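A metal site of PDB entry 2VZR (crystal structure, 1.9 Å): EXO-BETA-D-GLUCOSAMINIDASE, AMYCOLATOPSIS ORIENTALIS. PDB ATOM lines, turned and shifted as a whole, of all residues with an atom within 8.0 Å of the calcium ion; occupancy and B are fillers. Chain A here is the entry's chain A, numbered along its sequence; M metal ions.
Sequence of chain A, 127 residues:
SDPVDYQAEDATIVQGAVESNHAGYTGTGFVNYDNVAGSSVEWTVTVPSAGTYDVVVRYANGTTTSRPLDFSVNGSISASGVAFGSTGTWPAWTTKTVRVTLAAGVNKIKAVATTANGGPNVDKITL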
ATOM      1  N   TYR A   6     -23.512 -15.607   4.978  1.00  0.00           N
ATOM      2  CA  TYR A   6     -22.714 -15.205   3.834  1.00  0.00           C
ATOM      3  C   TYR A   6     -23.643 -15.091   2.616  1.00  0.00           C
ATOM      4  O   TYR A   6     -24.004 -16.091   2.004  1.00  0.00           O
ATOM      5  CB  TYR A   6     -21.610 -16.241   3.572  1.00  0.00           C
ATOM      6  CG  TYR A   6     -20.590 -16.394   4.696  1.00  0.00           C
ATOM      7  CD1 TYR A   6     -20.741 -17.391   5.664  1.00  0.00           C
ATOM      8  CD2 TYR A   6     -19.459 -15.570   4.772  1.00  0.00           C
ATOM      9  CE1 TYR A   6     -19.801 -17.561   6.698  1.00  0.00           C
ATOM     10  CE2 TYR A   6     -18.518 -15.720   5.809  1.00  0.00           C
ATOM     11  CZ  TYR A   6     -18.710 -16.714   6.767  1.00  0.00           C
ATOM     12  OH  TYR A   6     -17.792 -16.890   7.778  1.00  0.00           O
ATOM     13  N   GLN A   7     -24.034 -13.866   2.278  1.00  0.00           N
ATOM     14  CA  GLN A   7     -24.957 -13.605   1.161  1.00  0.00           C
ATOM     15  C   GLN A   7     -24.446 -14.022  -0.226  1.00  0.00           C
ATOM     16  O   GLN A   7     -23.310 -13.722  -0.599  1.00  0.00           O
ATOM     17  CB  GLN A   7     -25.385 -12.125   1.177  1.00  0.00           C
ATOM     18  CG  GLN A   7     -26.069 -11.693   2.485  1.00  0.00           C
ATOM     19  CD  GLN A   7     -27.379 -12.426   2.725  1.00  0.00           C
ATOM     20  OE1 GLN A   7     -28.000 -12.942   1.785  1.00  0.00           O
ATOM     21  NE2 GLN A   7     -27.835 -12.468   3.992  1.00  0.00           N
ATOM     22  N   ALA A   8     -25.285 -14.718  -0.996  1.00  0.00           N
ATOM     23  CA  ALA A   8     -24.888 -15.211  -2.328  1.00  0.00           C
ATOM     24  C   ALA A   8     -24.533 -14.061  -3.270  1.00  0.00           C
ATOM     25  O   ALA A   8     -23.568 -14.145  -4.057  1.00  0.00           O
ATOM     26  CB  ALA A   8     -26.016 -16.077  -2.920  1.00  0.00           C
ATOM     27  N   GLU A   9     -25.315 -12.987  -3.186  1.00  0.00           N
ATOM     28  CA  GLU A   9     -25.140 -11.787  -4.013  1.00  0.00           C
ATOM     29  C   GLU A   9     -23.813 -11.067  -3.721  1.00  0.00           C
ATOM     30  O   GLU A   9     -23.413 -10.176  -4.468  1.00  0.00           O
ATOM     31  CB  GLU A   9     -26.324 -10.820  -3.825  1.00  0.00           C
ATOM     32  CG  GLU A   9     -26.557 -10.284  -2.389  1.00  0.00           C
ATOM     33  CD  GLU A   9     -27.490 -11.147  -1.546  1.00  0.00           C
ATOM     34  OE1 GLU A   9     -27.648 -12.373  -1.783  1.00  0.00           O
ATOM     35  OE2 GLU A   9     -28.076 -10.617  -0.606  1.00  0.00           O
ATOM     36  N   ASP A  10     -23.147 -11.450  -2.631  1.00  0.00           N
ATOM     37  CA  ASP A  10     -21.857 -10.882  -2.252  1.00  0.00           C
ATOM     38  C   ASP A  10     -20.695 -11.809  -2.584  1.00  0.00           C
ATOM     39  O   ASP A  10     -19.528 -11.484  -2.403  1.00  0.00           O
ATOM     40  CB  ASP A  10     -21.866 -10.530  -0.756  1.00  0.00           C
ATOM     41  CG  ASP A  10     -22.890  -9.444  -0.422  1.00  0.00           C
ATOM     42  OD1 ASP A  10     -23.051  -8.486  -1.207  1.00  0.00           O
ATOM     43  OD2 ASP A  10     -23.537  -9.545   0.635  1.00  0.00           O
ATOM     44  N   VAL A  18     -27.468 -11.227  -9.866  1.00  0.00           N
ATOM     45  CA  VAL A  18     -28.118 -10.736  -8.635  1.00  0.00           C
ATOM     46  C   VAL A  18     -29.504 -10.166  -8.979  1.00  0.00           C
ATOM     47  O   VAL A  18     -29.626  -9.264  -9.807  1.00  0.00           O
ATOM     48  CB  VAL A  18     -27.226  -9.705  -7.886  1.00  0.00           C
ATOM     49  CG1 VAL A  18     -27.971  -9.075  -6.687  1.00  0.00           C
ATOM     50  CG2 VAL A  18     -25.930 -10.378  -7.431  1.00  0.00           C
ATOM     51  N   GLU A  19     -30.534 -10.725  -8.353  1.00  0.00           N
ATOM     52  CA  GLU A  19     -31.907 -10.301  -8.595  1.00  0.00           C
ATOM     53  C   GLU A  19     -32.616 -10.164  -7.268  1.00  0.00           C
ATOM     54  O   GLU A  19     -32.084 -10.549  -6.226  1.00  0.00           O
ATOM     55  CB  GLU A  19     -32.610 -11.265  -9.566  1.00  0.00           C
ATOM     56  CG  GLU A  19     -31.837 -11.342 -10.897  1.00  0.00           C
ATOM     57  CD  GLU A  19     -32.515 -12.118 -11.991  1.00  0.00           C
ATOM     58  OE1 GLU A  19     -33.420 -12.925 -11.717  1.00  0.00           O
ATOM     59  OE2 GLU A  19     -32.097 -11.908 -13.155  1.00  0.00           O
ATOM     60  N   GLY A  24     -38.673 -12.300   0.209  1.00  0.00           N
ATOM     61  CA  GLY A  24     -38.256 -13.220   1.271  1.00  0.00           C
ATOM     62  C   GLY A  24     -36.769 -13.445   1.370  1.00  0.00           C
ATOM     63  O   GLY A  24     -36.303 -14.086   2.299  1.00  0.00           O
ATOM     64  N   TYR A  25     -36.015 -12.925   0.400  1.00  0.00           N
ATOM     65  CA  TYR A  25     -34.568 -13.001   0.450  1.00  0.00           C
ATOM     66  C   TYR A  25     -34.047 -12.164   1.640  1.00  0.00           C
ATOM     67  O   TYR A  25     -34.760 -11.280   2.147  1.00  0.00           O
ATOM     68  CB  TYR A  25     -33.935 -12.549  -0.888  1.00  0.00           C
ATOM     69  CG  TYR A  25     -34.308 -11.127  -1.272  1.00  0.00           C
ATOM     70  CD1 TYR A  25     -33.631 -10.033  -0.731  1.00  0.00           C
ATOM     71  CD2 TYR A  25     -35.361 -10.884  -2.163  1.00  0.00           C
ATOM     72  CE1 TYR A  25     -33.980  -8.718  -1.070  1.00  0.00           C
ATOM     73  CE2 TYR A  25     -35.714  -9.567  -2.516  1.00  0.00           C
ATOM     74  CZ  TYR A  25     -35.006  -8.487  -1.949  1.00  0.00           C
ATOM     75  OH  TYR A  25     -35.338  -7.177  -2.256  1.00  0.00           O
ATOM     76  N   THR A  26     -32.854 -12.502   2.092  1.00  0.00           N
ATOM     77  CA  THR A  26     -32.112 -11.716   3.108  1.00  0.00           C
ATOM     78  C   THR A  26     -30.952 -11.029   2.408  1.00  0.00           C
ATOM     79  O   THR A  26     -30.674 -11.319   1.232  1.00  0.00           O
ATOM     80  CB  THR A  26     -31.601 -12.600   4.258  1.00  0.00           C
ATOM     81  OG1 THR A  26     -30.766 -13.655   3.726  1.00  0.00           O
ATOM     82  CG2 THR A  26     -32.756 -13.213   5.004  1.00  0.00           C
ATOM     83  N   GLY A  27     -30.285 -10.096   3.094  1.00  0.00           N
ATOM     84  CA  GLY A  27     -29.297  -9.255   2.402  1.00  0.00           C
ATOM     85  C   GLY A  27     -29.988  -8.356   1.386  1.00  0.00           C
ATOM     86  O   GLY A  27     -31.160  -8.021   1.547  1.00  0.00           O
ATOM     87  N   THR A  28     -29.281  -8.003   0.324  1.00  0.00           N
ATOM     88  CA  THR A  28     -29.848  -7.083  -0.646  1.00  0.00           C
ATOM     89  C   THR A  28     -30.514  -7.786  -1.838  1.00  0.00           C
ATOM     90  O   THR A  28     -31.102  -7.134  -2.683  1.00  0.00           O
ATOM     91  CB  THR A  28     -28.779  -6.089  -1.139  1.00  0.00           C
ATOM     92  OG1 THR A  28     -27.663  -6.819  -1.653  1.00  0.00           O
ATOM     93  CG2 THR A  28     -28.309  -5.204   0.006  1.00  0.00           C
ATOM     94  N   GLY A  29     -30.422  -9.112  -1.899  1.00  0.00           N
ATOM     95  CA  GLY A  29     -30.987  -9.855  -3.031  1.00  0.00           C
ATOM     96  C   GLY A  29     -30.722 -11.335  -2.951  1.00  0.00           C
ATOM     97  O   GLY A  29     -30.655 -11.897  -1.870  1.00  0.00           O
ATOM     98  N   PHE A  30     -30.604 -11.966  -4.117  1.00  0.00           N
ATOM     99  CA  PHE A  30     -30.246 -13.404  -4.210  1.00  0.00           C
ATOM    100  C   PHE A  30     -29.535 -13.632  -5.536  1.00  0.00           C
ATOM    101  O   PHE A  30     -29.540 -12.747  -6.395  1.00  0.00           O
ATOM    102  CB  PHE A  30     -31.482 -14.325  -4.080  1.00  0.00           C
ATOM    103  CG  PHE A  30     -32.612 -13.982  -5.023  1.00  0.00           C
ATOM    104  CD1 PHE A  30     -32.687 -14.543  -6.306  1.00  0.00           C
ATOM    105  CD2 PHE A  30     -33.624 -13.108  -4.618  1.00  0.00           C
ATOM    106  CE1 PHE A  30     -33.720 -14.222  -7.177  1.00  0.00           C
ATOM    107  CE2 PHE A  30     -34.684 -12.768  -5.479  1.00  0.00           C
ATOM    108  CZ  PHE A  30     -34.727 -13.320  -6.755  1.00  0.00           C
ATOM    109  N   VAL A  31     -28.941 -14.814  -5.688  1.00  0.00           N
ATOM    110  CA  VAL A  31     -28.400 -15.215  -6.977  1.00  0.00           C
ATOM    111  C   VAL A  31     -29.369 -16.110  -7.750  1.00  0.00           C
ATOM    112  O   VAL A  31     -29.816 -17.143  -7.286  1.00  0.00           O
ATOM    113  CB  VAL A  31     -26.994 -15.882  -6.885  1.00  0.00           C
ATOM    114  CG1 VAL A  31     -26.528 -16.318  -8.276  1.00  0.00           C
ATOM    115  CG2 VAL A  31     -26.006 -14.897  -6.330  1.00  0.00           C
ATOM    116  N   TRP A  43     -18.505 -18.787  -2.298  1.00  0.00           N
ATOM    117  CA  TRP A  43     -18.428 -17.997  -1.065  1.00  0.00           C
ATOM    118  C   TRP A  43     -17.036 -18.071  -0.428  1.00  0.00           C
ATOM    119  O   TRP A  43     -16.388 -19.122  -0.445  1.00  0.00           O
ATOM    120  CB  TRP A  43     -19.437 -18.520  -0.037  1.00  0.00           C
ATOM    121  CG  TRP A  43     -20.885 -18.314  -0.369  1.00  0.00           C
ATOM    122  CD1 TRP A  43     -21.670 -17.274   0.041  1.00  0.00           C
ATOM    123  CD2 TRP A  43     -21.729 -19.195  -1.119  1.00  0.00           C
ATOM    124  NE1 TRP A  43     -22.954 -17.446  -0.433  1.00  0.00           N
ATOM    125  CE2 TRP A  43     -23.012 -18.598  -1.155  1.00  0.00           C
ATOM    126  CE3 TRP A  43     -21.516 -20.397  -1.806  1.00  0.00           C
ATOM    127  CZ2 TRP A  43     -24.074 -19.182  -1.825  1.00  0.00           C
ATOM    128  CZ3 TRP A  43     -22.596 -20.993  -2.464  1.00  0.00           C
ATOM    129  CH2 TRP A  43     -23.857 -20.371  -2.473  1.00  0.00           C
ATOM    130  N   ARG A  58     -29.802 -21.536   1.860  1.00  0.00           N
ATOM    131  CA  ARG A  58     -31.165 -21.006   1.728  1.00  0.00           C
ATOM    132  C   ARG A  58     -31.447 -20.738   0.247  1.00  0.00           C
ATOM    133  O   ARG A  58     -30.746 -19.938  -0.398  1.00  0.00           O
ATOM    134  CB  ARG A  58     -31.375 -19.744   2.572  1.00  0.00           C
ATOM    135  CG  ARG A  58     -32.843 -19.274   2.673  1.00  0.00           C
ATOM    136  CD  ARG A  58     -33.014 -18.254   3.815  1.00  0.00           C
ATOM    137  NE  ARG A  58     -34.434 -17.936   4.059  1.00  0.00           N
ATOM    138  CZ  ARG A  58     -35.063 -16.850   3.588  1.00  0.00           C
ATOM    139  NH1 ARG A  58     -34.426 -15.954   2.843  1.00  0.00           N
ATOM    140  NH2 ARG A  58     -36.353 -16.662   3.885  1.00  0.00           N
ATOM    141  N   TRP A  93     -38.735 -19.560   0.234  1.00  0.00           N
ATOM    142  CA  TRP A  93     -37.368 -19.970   0.600  1.00  0.00           C
ATOM    143  C   TRP A  93     -37.327 -21.093   1.653  1.00  0.00           C
ATOM    144  O   TRP A  93     -38.037 -21.074   2.657  1.00  0.00           O
ATOM    145  CB  TRP A  93     -36.557 -18.763   1.100  1.00  0.00           C
ATOM    146  CG  TRP A  93     -36.497 -17.637   0.089  1.00  0.00           C
ATOM    147  CD1 TRP A  93     -37.361 -16.565  -0.018  1.00  0.00           C
ATOM    148  CD2 TRP A  93     -35.540 -17.483  -0.967  1.00  0.00           C
ATOM    149  NE1 TRP A  93     -36.980 -15.754  -1.069  1.00  0.00           N
ATOM    150  CE2 TRP A  93     -35.863 -16.292  -1.661  1.00  0.00           C
ATOM    151  CE3 TRP A  93     -34.422 -18.236  -1.380  1.00  0.00           C
ATOM    152  CZ2 TRP A  93     -35.118 -15.844  -2.758  1.00  0.00           C
ATOM    153  CZ3 TRP A  93     -33.682 -17.790  -2.469  1.00  0.00           C
ATOM    154  CH2 TRP A  93     -34.037 -16.601  -3.146  1.00  0.00           C
ATOM    155  N   VAL A 122     -30.454 -18.917  -5.057  1.00  0.00           N
ATOM    156  CA  VAL A 122     -29.773 -19.077  -3.760  1.00  0.00           C
ATOM    157  C   VAL A 122     -29.693 -17.732  -3.048  1.00  0.00           C
ATOM    158  O   VAL A 122     -29.222 -16.746  -3.609  1.00  0.00           O
ATOM    159  CB  VAL A 122     -28.350 -19.736  -3.874  1.00  0.00           C
ATOM    160  CG1 VAL A 122     -27.656 -19.815  -2.503  1.00  0.00           C
ATOM    161  CG2 VAL A 122     -28.425 -21.143  -4.500  1.00  0.00           C
ATOM    162  N   ASP A 123     -30.183 -17.698  -1.812  1.00  0.00           N
ATOM    163  CA  ASP A 123     -30.196 -16.472  -1.027  1.00  0.00           C
ATOM    164  C   ASP A 123     -28.839 -16.260  -0.339  1.00  0.00           C
ATOM    165  O   ASP A 123     -28.268 -15.176  -0.379  1.00  0.00           O
ATOM    166  CB  ASP A 123     -31.365 -16.537  -0.004  1.00  0.00           C
ATOM    167  CG  ASP A 123     -31.417 -15.322   0.941  1.00  0.00           C
ATOM    168  OD1 ASP A 123     -31.196 -14.186   0.494  1.00  0.00           O
ATOM    169  OD2 ASP A 123     -31.733 -15.527   2.125  1.00  0.00           O
ATOM    170  N   LYS A 124     -28.328 -17.323   0.277  1.00  0.00           N
ATOM    171  CA  LYS A 124     -27.147 -17.270   1.125  1.00  0.00           C
ATOM    172  C   LYS A 124     -26.784 -18.681   1.573  1.00  0.00           C
ATOM    173  O   LYS A 124     -27.540 -19.636   1.361  1.00  0.00           O
ATOM    174  CB  LYS A 124     -27.413 -16.416   2.378  1.00  0.00           C
ATOM    175  CG  LYS A 124     -28.585 -16.923   3.242  1.00  0.00           C
ATOM    176  CD  LYS A 124     -28.678 -16.190   4.617  1.00  0.00           C
ATOM    177  CE  LYS A 124     -30.020 -16.482   5.258  1.00  0.00           C
ATOM    178  NZ  LYS A 124     -30.286 -15.774   6.549  1.00  0.00           N
ATOM    179  N   ILE A 125     -25.612 -18.799   2.191  1.00  0.00           N
ATOM    180  CA  ILE A 125     -25.272 -19.950   3.035  1.00  0.00           C
ATOM    181  C   ILE A 125     -24.994 -19.440   4.441  1.00  0.00           C
ATOM    182  O   ILE A 125     -24.600 -18.272   4.626  1.00  0.00           O
ATOM    183  CB  ILE A 125     -24.061 -20.812   2.509  1.00  0.00           C
ATOM    184  CG1 ILE A 125     -22.732 -20.000   2.507  1.00  0.00           C
ATOM    185  CG2 ILE A 125     -24.396 -21.438   1.149  1.00  0.00           C
ATOM    186  CD1 ILE A 125     -21.453 -20.869   2.176  1.00  0.00           C
HETATM  187 CA    CA M   1     -29.333 -12.802  -0.088  1.00  0.00          CA
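The backbone NH of Thr 28 sits close to the side-chain carboxylate of Glu 9 (3.0 Å). OD2 of Asp 123 lies within salt-bridge range of NH1 of Arg 58 (2.8 Å). N of Ala 8 sits close to O of Asp 123, at 3.1 Å.
Within 4 Å of the calcium ion: Gln 7, Glu 9, Thr 26, Gly 29 and Asp 123. The nearest printed residue that does not touch the calcium ion is Phe 30 (4.3 Å).
The calcium ion is bound by OE1 of Gln 7, OD1 of Asp 123, O of Thr 26, O of Gly 29, OE1 of Glu 9, OE2 of Glu 9 and O of Asp 123.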
